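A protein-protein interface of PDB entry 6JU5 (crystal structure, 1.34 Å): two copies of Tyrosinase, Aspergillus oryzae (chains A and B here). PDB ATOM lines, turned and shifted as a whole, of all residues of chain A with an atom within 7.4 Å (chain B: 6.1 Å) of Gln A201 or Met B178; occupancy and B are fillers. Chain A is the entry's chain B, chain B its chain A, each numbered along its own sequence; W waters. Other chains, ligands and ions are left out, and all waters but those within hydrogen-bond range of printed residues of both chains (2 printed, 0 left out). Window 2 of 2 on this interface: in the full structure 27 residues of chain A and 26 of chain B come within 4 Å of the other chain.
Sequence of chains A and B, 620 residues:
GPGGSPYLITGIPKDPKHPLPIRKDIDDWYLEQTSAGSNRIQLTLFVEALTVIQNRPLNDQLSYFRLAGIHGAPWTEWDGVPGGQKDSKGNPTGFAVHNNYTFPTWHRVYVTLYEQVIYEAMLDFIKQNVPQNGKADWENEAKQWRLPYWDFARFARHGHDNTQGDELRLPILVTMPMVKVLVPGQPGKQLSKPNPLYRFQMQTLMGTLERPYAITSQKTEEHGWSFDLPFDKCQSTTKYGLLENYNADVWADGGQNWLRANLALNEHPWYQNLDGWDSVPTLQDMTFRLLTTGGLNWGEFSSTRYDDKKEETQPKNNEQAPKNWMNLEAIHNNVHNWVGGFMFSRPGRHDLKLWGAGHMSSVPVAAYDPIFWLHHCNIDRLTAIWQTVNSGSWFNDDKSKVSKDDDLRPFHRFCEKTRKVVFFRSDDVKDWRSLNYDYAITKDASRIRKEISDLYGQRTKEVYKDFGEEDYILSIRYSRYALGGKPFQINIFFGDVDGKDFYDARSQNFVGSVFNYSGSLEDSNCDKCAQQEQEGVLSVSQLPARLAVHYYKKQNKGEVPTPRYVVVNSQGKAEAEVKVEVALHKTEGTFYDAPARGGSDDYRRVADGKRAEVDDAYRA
The side-chain sulfur of Met B178 sits close to the side-chain amide oxygen of Gln A201 (3.5 Å). OG of Ser B192 is in hydrogen-bond range of NE2 of Gln A235.
Hydrophobic or aromatic side chains of chain B within 4 Å of the printed part of chain A: Met B176, Pro B177 and Met B178. Printed residues of chain A that touch a printed residue of chain B: Gln A201, Gln A203, Gln A235, Asp A249 and Asp A253. Among the printed residues, no Asp or Glu carboxylate lies within 4 Å of a Lys or Arg side-chain nitrogen of the other chain.
Ser B192 touches Gln A203. Asp A249 touches Met B176 (CB to SD, 3.9 Å). Asp A253 touches Pro B177.
The backbone carbonyl oxygen (O) of Met A202 is in hydrogen-bond range of the side-chain amide nitrogen (NE2) of Gln A235 (2.7 Å). NH2 of Arg A199 lies within hydrogen-bond range of OE1 of Gln A201. The backbone carbonyl oxygen (O) of Pro B177 is in hydrogen-bond range of the backbone NH (N) of Asn B195 (2.9 Å). OD2 of Asp A253 lies within salt-bridge range of NH1 of Arg A199. O of Ala A252 lies within hydrogen-bond range of N of Gln A235 (2.7 Å). The backbone carbonyl oxygen (O) of Met B176 sits at hydrogen-bond distance from the side-chain amide nitrogen (ND2) of Asn B195.
Water W2 lies within hydrogen-bond range of NE2 of Gln A201 (3.0 Å), SD of Met B178 (3.3 Å) and NH2 of Arg A199 (3.5 Å). Water W1 bridges NH2 of Arg A199 and SD of Met B178.
1 position is printed for both chains. Of the 5 pairs that touch across the chains among the printed residues, none has its exchanged pair printed and touching as well.
Of chain B, only Met B178 (3.5 Å) comes within 4 Å of Gln A201. Of the printed residues of chain B, Gln A235 touches Ser B192. Of the printed residues of chain B, Asp A249 touches Met B176 (3.9 Å). Printed residues of chain B within 4 Å of Asp A253: Pro B177 (3.2 Å). Printed residues of chain A within 4 Å of Met B176: Asp A249. Of chain A, only Gln A201 comes within 4 Å of Met B178. Of the printed residues of chain A, Ser B192 touches Gln A203 and Gln A235.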
ATOM      1  N   GLN A  54      -0.247  19.356 -11.630  1.00  0.00           N
ATOM      2  CA  GLN A  54       0.250  20.452 -12.465  1.00  0.00           C
ATOM      3  C   GLN A  54      -0.639  20.707 -13.681  1.00  0.00           C
ATOM      4  O   GLN A  54      -0.728  21.848 -14.167  1.00  0.00           O
ATOM      5  CB  GLN A  54       1.698  20.189 -12.909  1.00  0.00           C
ATOM      6  CG  GLN A  54       2.673  20.376 -11.757  1.00  0.00           C
ATOM      7  CD  GLN A  54       4.125  20.126 -12.129  1.00  0.00           C
ATOM      8  OE1 GLN A  54       4.427  19.588 -13.193  1.00  0.00           O
ATOM      9  NE2 GLN A  54       5.035  20.534 -11.250  1.00  0.00           N
ATOM     10  N   ASN A  55      -1.281  19.666 -14.202  1.00  0.00           N
ATOM     11  CA  ASN A  55      -2.115  19.803 -15.389  1.00  0.00           C
ATOM     12  C   ASN A  55      -3.553  20.164 -15.052  1.00  0.00           C
ATOM     13  O   ASN A  55      -4.367  20.335 -15.979  1.00  0.00           O
ATOM     14  CB  ASN A  55      -2.039  18.519 -16.243  1.00  0.00           C
ATOM     15  CG  ASN A  55      -0.696  18.422 -16.950  1.00  0.00           C
ATOM     16  OD1 ASN A  55      -0.114  19.430 -17.343  1.00  0.00           O
ATOM     17  ND2 ASN A  55      -0.199  17.207 -17.149  1.00  0.00           N
ATOM     18  N   TYR A  64      -1.902  22.752  -9.203  1.00  0.00           N
ATOM     19  CA  TYR A  64      -0.604  23.267  -8.794  1.00  0.00           C
ATOM     20  C   TYR A  64      -0.579  24.787  -8.846  1.00  0.00           C
ATOM     21  O   TYR A  64      -0.077  25.458  -7.946  1.00  0.00           O
ATOM     22  CB  TYR A  64       0.493  22.704  -9.698  1.00  0.00           C
ATOM     23  CG  TYR A  64       1.908  23.049  -9.276  1.00  0.00           C
ATOM     24  CD1 TYR A  64       2.517  24.214  -9.762  1.00  0.00           C
ATOM     25  CD2 TYR A  64       2.645  22.224  -8.435  1.00  0.00           C
ATOM     26  CE1 TYR A  64       3.811  24.526  -9.393  1.00  0.00           C
ATOM     27  CE2 TYR A  64       3.939  22.536  -8.049  1.00  0.00           C
ATOM     28  CZ  TYR A  64       4.512  23.699  -8.531  1.00  0.00           C
ATOM     29  OH  TYR A  64       5.800  23.990  -8.148  1.00  0.00           O
ATOM     30  N   PRO A 194       8.164  13.582 -18.858  1.00  0.00           N
ATOM     31  CA  PRO A 194       8.686  14.870 -18.372  1.00  0.00           C
ATOM     32  C   PRO A 194       8.613  14.893 -16.850  1.00  0.00           C
ATOM     33  O   PRO A 194       7.633  14.475 -16.244  1.00  0.00           O
ATOM     34  CB  PRO A 194       7.759  15.910 -18.999  1.00  0.00           C
ATOM     35  CG  PRO A 194       7.302  15.197 -20.255  1.00  0.00           C
ATOM     36  CD  PRO A 194       7.029  13.776 -19.771  1.00  0.00           C
ATOM     37  N   PRO A 196       8.030  16.387 -13.372  1.00  0.00           N
ATOM     38  CA  PRO A 196       7.310  17.545 -12.827  1.00  0.00           C
ATOM     39  C   PRO A 196       8.116  18.273 -11.757  1.00  0.00           C
ATOM     40  O   PRO A 196       7.695  19.356 -11.331  1.00  0.00           O
ATOM     41  CB  PRO A 196       6.050  16.903 -12.234  1.00  0.00           C
ATOM     42  CG  PRO A 196       6.504  15.536 -11.838  1.00  0.00           C
ATOM     43  CD  PRO A 196       7.444  15.109 -12.947  1.00  0.00           C
ATOM     44  N   ARG A 199      10.587  21.637 -13.561  1.00  0.00           N
ATOM     45  CA  ARG A 199       9.987  22.924 -13.842  1.00  0.00           C
ATOM     46  C   ARG A 199       8.473  22.788 -13.719  1.00  0.00           C
ATOM     47  O   ARG A 199       7.964  21.676 -13.784  1.00  0.00           O
ATOM     48  CB  ARG A 199      10.321  23.427 -15.255  1.00  0.00           C
ATOM     49  CG  ARG A 199       9.693  22.583 -16.347  1.00  0.00           C
ATOM     50  CD  ARG A 199      10.008  23.118 -17.750  1.00  0.00           C
ATOM     51  NE  ARG A 199       9.481  22.142 -18.713  1.00  0.00           N
ATOM     52  CZ  ARG A 199       9.868  21.969 -19.956  1.00  0.00           C
ATOM     53  NH1 ARG A 199      10.828  22.749 -20.456  1.00  0.00           N
ATOM     54  NH2 ARG A 199       9.324  21.025 -20.708  1.00  0.00           N
ATOM     55  N   PHE A 200       7.818  23.931 -13.592  1.00  0.00           N
ATOM     56  CA  PHE A 200       6.371  23.993 -13.809  1.00  0.00           C
ATOM     57  C   PHE A 200       6.111  24.802 -15.081  1.00  0.00           C
ATOM     58  O   PHE A 200       6.588  25.931 -15.193  1.00  0.00           O
ATOM     59  CB  PHE A 200       5.692  24.644 -12.600  1.00  0.00           C
ATOM     60  CG  PHE A 200       4.212  24.876 -12.825  1.00  0.00           C
ATOM     61  CD1 PHE A 200       3.353  23.846 -13.146  1.00  0.00           C
ATOM     62  CD2 PHE A 200       3.667  26.147 -12.720  1.00  0.00           C
ATOM     63  CE1 PHE A 200       1.996  24.055 -13.355  1.00  0.00           C
ATOM     64  CE2 PHE A 200       2.318  26.374 -12.920  1.00  0.00           C
ATOM     65  CZ  PHE A 200       1.465  25.326 -13.215  1.00  0.00           C
ATOM     66  N   GLN A 201       5.415  24.206 -16.021  1.00  0.00           N
ATOM     67  CA  GLN A 201       5.118  24.822 -17.320  1.00  0.00           C
ATOM     68  C   GLN A 201       3.613  24.986 -17.480  1.00  0.00           C
ATOM     69  O   GLN A 201       2.867  24.035 -17.239  1.00  0.00           O
ATOM     70  CB  GLN A 201       5.700  23.929 -18.423  1.00  0.00           C
ATOM     71  CG  GLN A 201       5.374  24.242 -19.863  1.00  0.00           C
ATOM     72  CD  GLN A 201       5.937  23.196 -20.807  1.00  0.00           C
ATOM     73  OE1 GLN A 201       6.999  23.395 -21.406  1.00  0.00           O
ATOM     74  NE2 GLN A 201       5.236  22.085 -20.950  1.00  0.00           N
ATOM     75  N   MET A 202       3.162  26.157 -17.881  1.00  0.00           N
ATOM     76  CA  MET A 202       1.779  26.378 -18.306  1.00  0.00           C
ATOM     77  C   MET A 202       1.618  26.363 -19.813  1.00  0.00           C
ATOM     78  O   MET A 202       2.610  26.206 -20.519  1.00  0.00           O
ATOM     79  CB  MET A 202       1.331  27.743 -17.768  1.00  0.00           C
ATOM     80  CG  MET A 202       1.816  27.809 -16.304  1.00  0.00           C
ATOM     81  SD  MET A 202       0.714  28.892 -15.403  1.00  0.00           S
ATOM     82  CE  MET A 202      -0.738  27.817 -15.327  1.00  0.00           C
ATOM     83  N   GLN A 203       0.389  26.508 -20.306  1.00  0.00           N
ATOM     84  CA  GLN A 203       0.176  26.365 -21.746  1.00  0.00           C
ATOM     85  C   GLN A 203       0.408  27.658 -22.504  1.00  0.00           C
ATOM     86  O   GLN A 203       0.466  27.707 -23.732  1.00  0.00           O
ATOM     87  CB  GLN A 203      -1.256  25.874 -21.984  1.00  0.00           C
ATOM     88  CG  GLN A 203      -1.561  24.633 -21.151  1.00  0.00           C
ATOM     89  CD  GLN A 203      -3.049  24.359 -21.064  1.00  0.00           C
ATOM     90  OE1 GLN A 203      -3.536  23.814 -20.073  1.00  0.00           O
ATOM     91  NE2 GLN A 203      -3.760  24.737 -22.120  1.00  0.00           N
ATOM     92  N   THR A 204       0.497  28.741 -21.732  1.00  0.00           N
ATOM     93  CA  THR A 204       0.741  30.055 -22.321  1.00  0.00           C
ATOM     94  C   THR A 204       1.583  30.902 -21.385  1.00  0.00           C
ATOM     95  O   THR A 204       1.866  30.477 -20.249  1.00  0.00           O
ATOM     96  CB  THR A 204      -0.589  30.754 -22.644  1.00  0.00           C
ATOM     97  OG1 THR A 204      -0.290  31.973 -23.337  1.00  0.00           O
ATOM     98  CG2 THR A 204      -1.332  31.081 -21.358  1.00  0.00           C
ATOM     99  N   MET A 206       2.485  33.415 -18.567  1.00  0.00           N
ATOM    100  CA  MET A 206       1.675  33.578 -17.354  1.00  0.00           C
ATOM    101  C   MET A 206       1.057  34.969 -17.289  1.00  0.00           C
ATOM    102  O   MET A 206       0.044  35.145 -16.612  1.00  0.00           O
ATOM    103  CB  MET A 206       2.541  33.303 -16.124  1.00  0.00           C
ATOM    104  CG  MET A 206       2.970  31.825 -16.037  1.00  0.00           C
ATOM    105  SD  MET A 206       3.653  31.511 -14.399  1.00  0.00           S
ATOM    106  CE  MET A 206       4.556  29.981 -14.674  1.00  0.00           C
ATOM    107  N   GLN A 235       6.413  31.284 -19.565  1.00  0.00           N
ATOM    108  CA  GLN A 235       5.479  30.172 -19.562  1.00  0.00           C
ATOM    109  C   GLN A 235       5.869  29.116 -18.535  1.00  0.00           C
ATOM    110  O   GLN A 235       5.018  28.442 -17.968  1.00  0.00           O
ATOM    111  CB  GLN A 235       5.472  29.563 -20.970  1.00  0.00           C
ATOM    112  CG  GLN A 235       4.631  28.315 -21.135  1.00  0.00           C
ATOM    113  CD  GLN A 235       4.731  27.756 -22.544  1.00  0.00           C
ATOM    114  OE1 GLN A 235       5.357  28.354 -23.426  1.00  0.00           O
ATOM    115  NE2 GLN A 235       4.129  26.596 -22.767  1.00  0.00           N
ATOM    116  N   SER A 236       7.170  28.943 -18.329  1.00  0.00           N
ATOM    117  CA  SER A 236       7.723  27.996 -17.369  1.00  0.00           C
ATOM    118  C   SER A 236       8.602  28.714 -16.347  1.00  0.00           C
ATOM    119  O   SER A 236       9.179  29.778 -16.598  1.00  0.00           O
ATOM    120  CB  SER A 236       8.559  26.923 -18.081  1.00  0.00           C
ATOM    121  OG  SER A 236       7.687  26.052 -18.802  1.00  0.00           O
ATOM    122  N   THR A 237       8.722  28.067 -15.201  1.00  0.00           N
ATOM    123  CA  THR A 237       9.668  28.492 -14.183  1.00  0.00           C
ATOM    124  C   THR A 237      11.089  28.294 -14.695  1.00  0.00           C
ATOM    125  O   THR A 237      11.361  27.431 -15.543  1.00  0.00           O
ATOM    126  CB  THR A 237       9.407  27.784 -12.848  1.00  0.00           C
ATOM    127  OG1 THR A 237       9.475  26.362 -13.040  1.00  0.00           O
ATOM    128  CG2 THR A 237       8.012  28.087 -12.317  1.00  0.00           C
ATOM    129  N   ASP A 249      11.234  36.036 -26.413  1.00  0.00           N
ATOM    130  CA  ASP A 249      10.703  34.670 -26.457  1.00  0.00           C
ATOM    131  C   ASP A 249      11.627  33.666 -25.773  1.00  0.00           C
ATOM    132  O   ASP A 249      11.184  32.569 -25.412  1.00  0.00           O
ATOM    133  CB  ASP A 249      10.409  34.230 -27.886  1.00  0.00           C
ATOM    134  CG  ASP A 249       9.320  35.057 -28.549  1.00  0.00           C
ATOM    135  OD1 ASP A 249       8.494  35.664 -27.849  1.00  0.00           O
ATOM    136  OD2 ASP A 249       9.300  35.083 -29.796  1.00  0.00           O
ATOM    137  N   ALA A 252      10.230  32.940 -22.307  1.00  0.00           N
ATOM    138  CA  ALA A 252       9.092  32.039 -22.097  1.00  0.00           C
ATOM    139  C   ALA A 252       9.534  30.818 -21.288  1.00  0.00           C
ATOM    140  O   ALA A 252       8.821  30.326 -20.421  1.00  0.00           O
ATOM    141  CB  ALA A 252       8.498  31.610 -23.439  1.00  0.00           C
ATOM    142  N   ASP A 253      10.715  30.291 -21.579  1.00  0.00           N
ATOM    143  CA  ASP A 253      11.287  29.208 -20.772  1.00  0.00           C
ATOM    144  C   ASP A 253      12.802  29.360 -20.811  1.00  0.00           C
ATOM    145  O   ASP A 253      13.476  28.994 -21.788  1.00  0.00           O
ATOM    146  CB  ASP A 253      10.847  27.841 -21.302  1.00  0.00           C
ATOM    147  CG  ASP A 253      11.393  26.707 -20.449  1.00  0.00           C
ATOM    148  OD1 ASP A 253      12.389  26.867 -19.708  1.00  0.00           O
ATOM    149  OD2 ASP A 253      10.833  25.599 -20.546  1.00  0.00           O
ATOM    150  N   TYR A 368       5.912  28.822  -7.616  1.00  0.00           N
ATOM    151  CA  TYR A 368       5.679  28.054  -8.842  1.00  0.00           C
ATOM    152  C   TYR A 368       6.829  27.097  -9.114  1.00  0.00           C
ATOM    153  O   TYR A 368       6.631  26.104  -9.808  1.00  0.00           O
ATOM    154  CB  TYR A 368       5.408  28.992 -10.044  1.00  0.00           C
ATOM    155  CG  TYR A 368       4.120  29.750  -9.806  1.00  0.00           C
ATOM    156  CD1 TYR A 368       2.890  29.117 -10.011  1.00  0.00           C
ATOM    157  CD2 TYR A 368       4.117  31.051  -9.327  1.00  0.00           C
ATOM    158  CE1 TYR A 368       1.689  29.777  -9.789  1.00  0.00           C
ATOM    159  CE2 TYR A 368       2.923  31.713  -9.074  1.00  0.00           C
ATOM    160  CZ  TYR A 368       1.717  31.073  -9.310  1.00  0.00           C
ATOM    161  OH  TYR A 368       0.519  31.709  -9.055  1.00  0.00           O
ATOM    162  N   PRO A 370       8.934  23.987  -8.666  1.00  0.00           N
ATOM    163  CA  PRO A 370       8.754  22.799  -7.828  1.00  0.00           C
ATOM    164  C   PRO A 370       9.767  22.659  -6.695  1.00  0.00           C
ATOM    165  O   PRO A 370       9.461  22.016  -5.673  1.00  0.00           O
ATOM    166  CB  PRO A 370       8.857  21.639  -8.834  1.00  0.00           C
ATOM    167  CG  PRO A 370       8.346  22.259 -10.111  1.00  0.00           C
ATOM    168  CD  PRO A 370       8.924  23.651 -10.108  1.00  0.00           C
ATOM    169  N   LEU B 173      16.088  30.829 -31.956  1.00  0.00           N
ATOM    170  CA  LEU B 173      15.133  29.705 -31.918  1.00  0.00           C
ATOM    171  C   LEU B 173      15.742  28.455 -31.299  1.00  0.00           C
ATOM    172  O   LEU B 173      15.055  27.652 -30.672  1.00  0.00           O
ATOM    173  CB  LEU B 173      14.658  29.467 -33.358  1.00  0.00           C
ATOM    174  CG  LEU B 173      13.548  28.453 -33.593  1.00  0.00           C
ATOM    175  CD1 LEU B 173      12.324  28.692 -32.742  1.00  0.00           C
ATOM    176  CD2 LEU B 173      13.189  28.465 -35.082  1.00  0.00           C
ATOM    177  N   MET B 176      15.239  28.173 -27.467  1.00  0.00           N
ATOM    178  CA  MET B 176      13.869  28.170 -26.949  1.00  0.00           C
ATOM    179  C   MET B 176      13.349  26.748 -26.765  1.00  0.00           C
ATOM    180  O   MET B 176      13.207  26.000 -27.739  1.00  0.00           O
ATOM    181  CB  MET B 176      12.932  28.933 -27.895  1.00  0.00           C
ATOM    182  CG  MET B 176      13.239  30.435 -28.009  1.00  0.00           C
ATOM    183  SD  MET B 176      12.379  31.217 -29.390  1.00  0.00           S
ATOM    184  CE  MET B 176      10.746  30.515 -29.225  1.00  0.00           C
ATOM    185  N   PRO B 177      13.060  26.327 -25.537  1.00  0.00           N
ATOM    186  CA  PRO B 177      12.471  24.993 -25.358  1.00  0.00           C
ATOM    187  C   PRO B 177      11.154  24.744 -26.083  1.00  0.00           C
ATOM    188  O   PRO B 177      10.875  23.608 -26.494  1.00  0.00           O
ATOM    189  CB  PRO B 177      12.267  24.926 -23.832  1.00  0.00           C
ATOM    190  CG  PRO B 177      13.359  25.813 -23.284  1.00  0.00           C
ATOM    191  CD  PRO B 177      13.417  26.967 -24.252  1.00  0.00           C
ATOM    192  N   MET B 178      10.298  25.749 -26.215  1.00  0.00           N
ATOM    193  CA  MET B 178       8.977  25.648 -26.817  1.00  0.00           C
ATOM    194  C   MET B 178       8.803  26.738 -27.873  1.00  0.00           C
ATOM    195  O   MET B 178       9.519  27.742 -27.800  1.00  0.00           O
ATOM    196  CB  MET B 178       7.846  25.832 -25.803  1.00  0.00           C
ATOM    197  CG  MET B 178       7.994  24.973 -24.562  1.00  0.00           C
ATOM    198  SD  MET B 178       7.591  23.240 -24.862  1.00  0.00           S
ATOM    199  CE  MET B 178       5.801  23.348 -24.976  1.00  0.00           C
ATOM    200  N   VAL B 179       7.860  26.520 -28.768  1.00  0.00           N
ATOM    201  CA  VAL B 179       7.600  27.512 -29.817  1.00  0.00           C
ATOM    202  C   VAL B 179       6.100  27.515 -30.079  1.00  0.00           C
ATOM    203  O   VAL B 179       5.468  26.454 -30.111  1.00  0.00           O
ATOM    204  CB  VAL B 179       8.410  27.221 -31.096  1.00  0.00           C
ATOM    205  CG1 VAL B 179       8.048  25.850 -31.634  1.00  0.00           C
ATOM    206  CG2 VAL B 179       8.191  28.314 -32.147  1.00  0.00           C
ATOM    207  N   LYS B 180       5.543  28.715 -30.214  1.00  0.00           N
ATOM    208  CA  LYS B 180       4.136  28.898 -30.528  1.00  0.00           C
ATOM    209  C   LYS B 180       3.919  28.726 -32.026  1.00  0.00           C
ATOM    210  O   LYS B 180       4.652  29.273 -32.854  1.00  0.00           O
ATOM    211  CB  LYS B 180       3.686  30.295 -30.077  1.00  0.00           C
ATOM    212  N   SER B 192       1.490  26.285 -27.970  1.00  0.00           N
ATOM    213  CA  SER B 192       2.900  26.145 -27.627  1.00  0.00           C
ATOM    214  C   SER B 192       3.332  24.694 -27.742  1.00  0.00           C
ATOM    215  O   SER B 192       2.683  23.847 -27.118  1.00  0.00           O
ATOM    216  CB  SER B 192       3.085  26.639 -26.186  1.00  0.00           C
ATOM    217  OG  SER B 192       4.440  26.547 -25.794  1.00  0.00           O
ATOM    218  N   LYS B 193       4.359  24.366 -28.512  1.00  0.00           N
ATOM    219  CA  LYS B 193       4.766  22.970 -28.646  1.00  0.00           C
ATOM    220  C   LYS B 193       6.260  22.826 -28.387  1.00  0.00           C
ATOM    221  O   LYS B 193       7.014  23.794 -28.563  1.00  0.00           O
ATOM    222  CB  LYS B 193       4.484  22.450 -30.057  1.00  0.00           C
ATOM    223  CG  LYS B 193       3.008  22.361 -30.390  1.00  0.00           C
ATOM    224  CD  LYS B 193       2.788  21.763 -31.768  1.00  0.00           C
ATOM    225  CE  LYS B 193       1.323  21.579 -32.100  1.00  0.00           C
ATOM    226  NZ  LYS B 193       1.148  20.435 -33.039  1.00  0.00           N
ATOM    227  N   PRO B 194       6.702  21.642 -28.004  1.00  0.00           N
ATOM    228  CA  PRO B 194       8.151  21.442 -27.857  1.00  0.00           C
ATOM    229  C   PRO B 194       8.842  21.791 -29.168  1.00  0.00           C
ATOM    230  O   PRO B 194       8.387  21.463 -30.269  1.00  0.00           O
ATOM    231  CB  PRO B 194       8.266  19.963 -27.515  1.00  0.00           C
ATOM    232  CG  PRO B 194       6.928  19.595 -26.934  1.00  0.00           C
ATOM    233  CD  PRO B 194       5.936  20.410 -27.728  1.00  0.00           C
ATOM    234  N   ASN B 195       9.949  22.511 -29.039  1.00  0.00           N
ATOM    235  CA  ASN B 195      10.685  22.981 -30.217  1.00  0.00           C
ATOM    236  C   ASN B 195      11.673  21.957 -30.731  1.00  0.00           C
ATOM    237  O   ASN B 195      12.611  21.593 -30.016  1.00  0.00           O
ATOM    238  CB  ASN B 195      11.465  24.238 -29.793  1.00  0.00           C
ATOM    239  CG  ASN B 195      12.261  24.866 -30.910  1.00  0.00           C
ATOM    240  OD1 ASN B 195      12.198  24.453 -32.072  1.00  0.00           O
ATOM    241  ND2 ASN B 195      13.040  25.890 -30.564  1.00  0.00           N
ATOM    242  N   TYR B 198      15.439  22.701 -30.574  1.00  0.00           N
ATOM    243  CA  TYR B 198      16.088  22.845 -29.260  1.00  0.00           C
ATOM    244  C   TYR B 198      16.937  21.633 -28.928  1.00  0.00           C
ATOM    245  O   TYR B 198      18.010  21.785 -28.326  1.00  0.00           O
ATOM    246  CB  TYR B 198      15.018  23.034 -28.207  1.00  0.00           C
ATOM    247  CG  TYR B 198      15.446  23.299 -26.789  1.00  0.00           C
ATOM    248  CD1 TYR B 198      16.050  24.497 -26.411  1.00  0.00           C
ATOM    249  CD2 TYR B 198      15.220  22.370 -25.786  1.00  0.00           C
ATOM    250  CE1 TYR B 198      16.425  24.717 -25.098  1.00  0.00           C
ATOM    251  CE2 TYR B 198      15.582  22.599 -24.460  1.00  0.00           C
ATOM    252  CZ  TYR B 198      16.196  23.780 -24.119  1.00  0.00           C
ATOM    253  OH  TYR B 198      16.544  24.018 -22.795  1.00  0.00           O
HETATM  254  O   HOH W   1       9.256  20.278 -23.729  1.00  0.00           O
HETATM  255  O   HOH W   2       6.738  20.604 -23.022  1.00  0.00           O
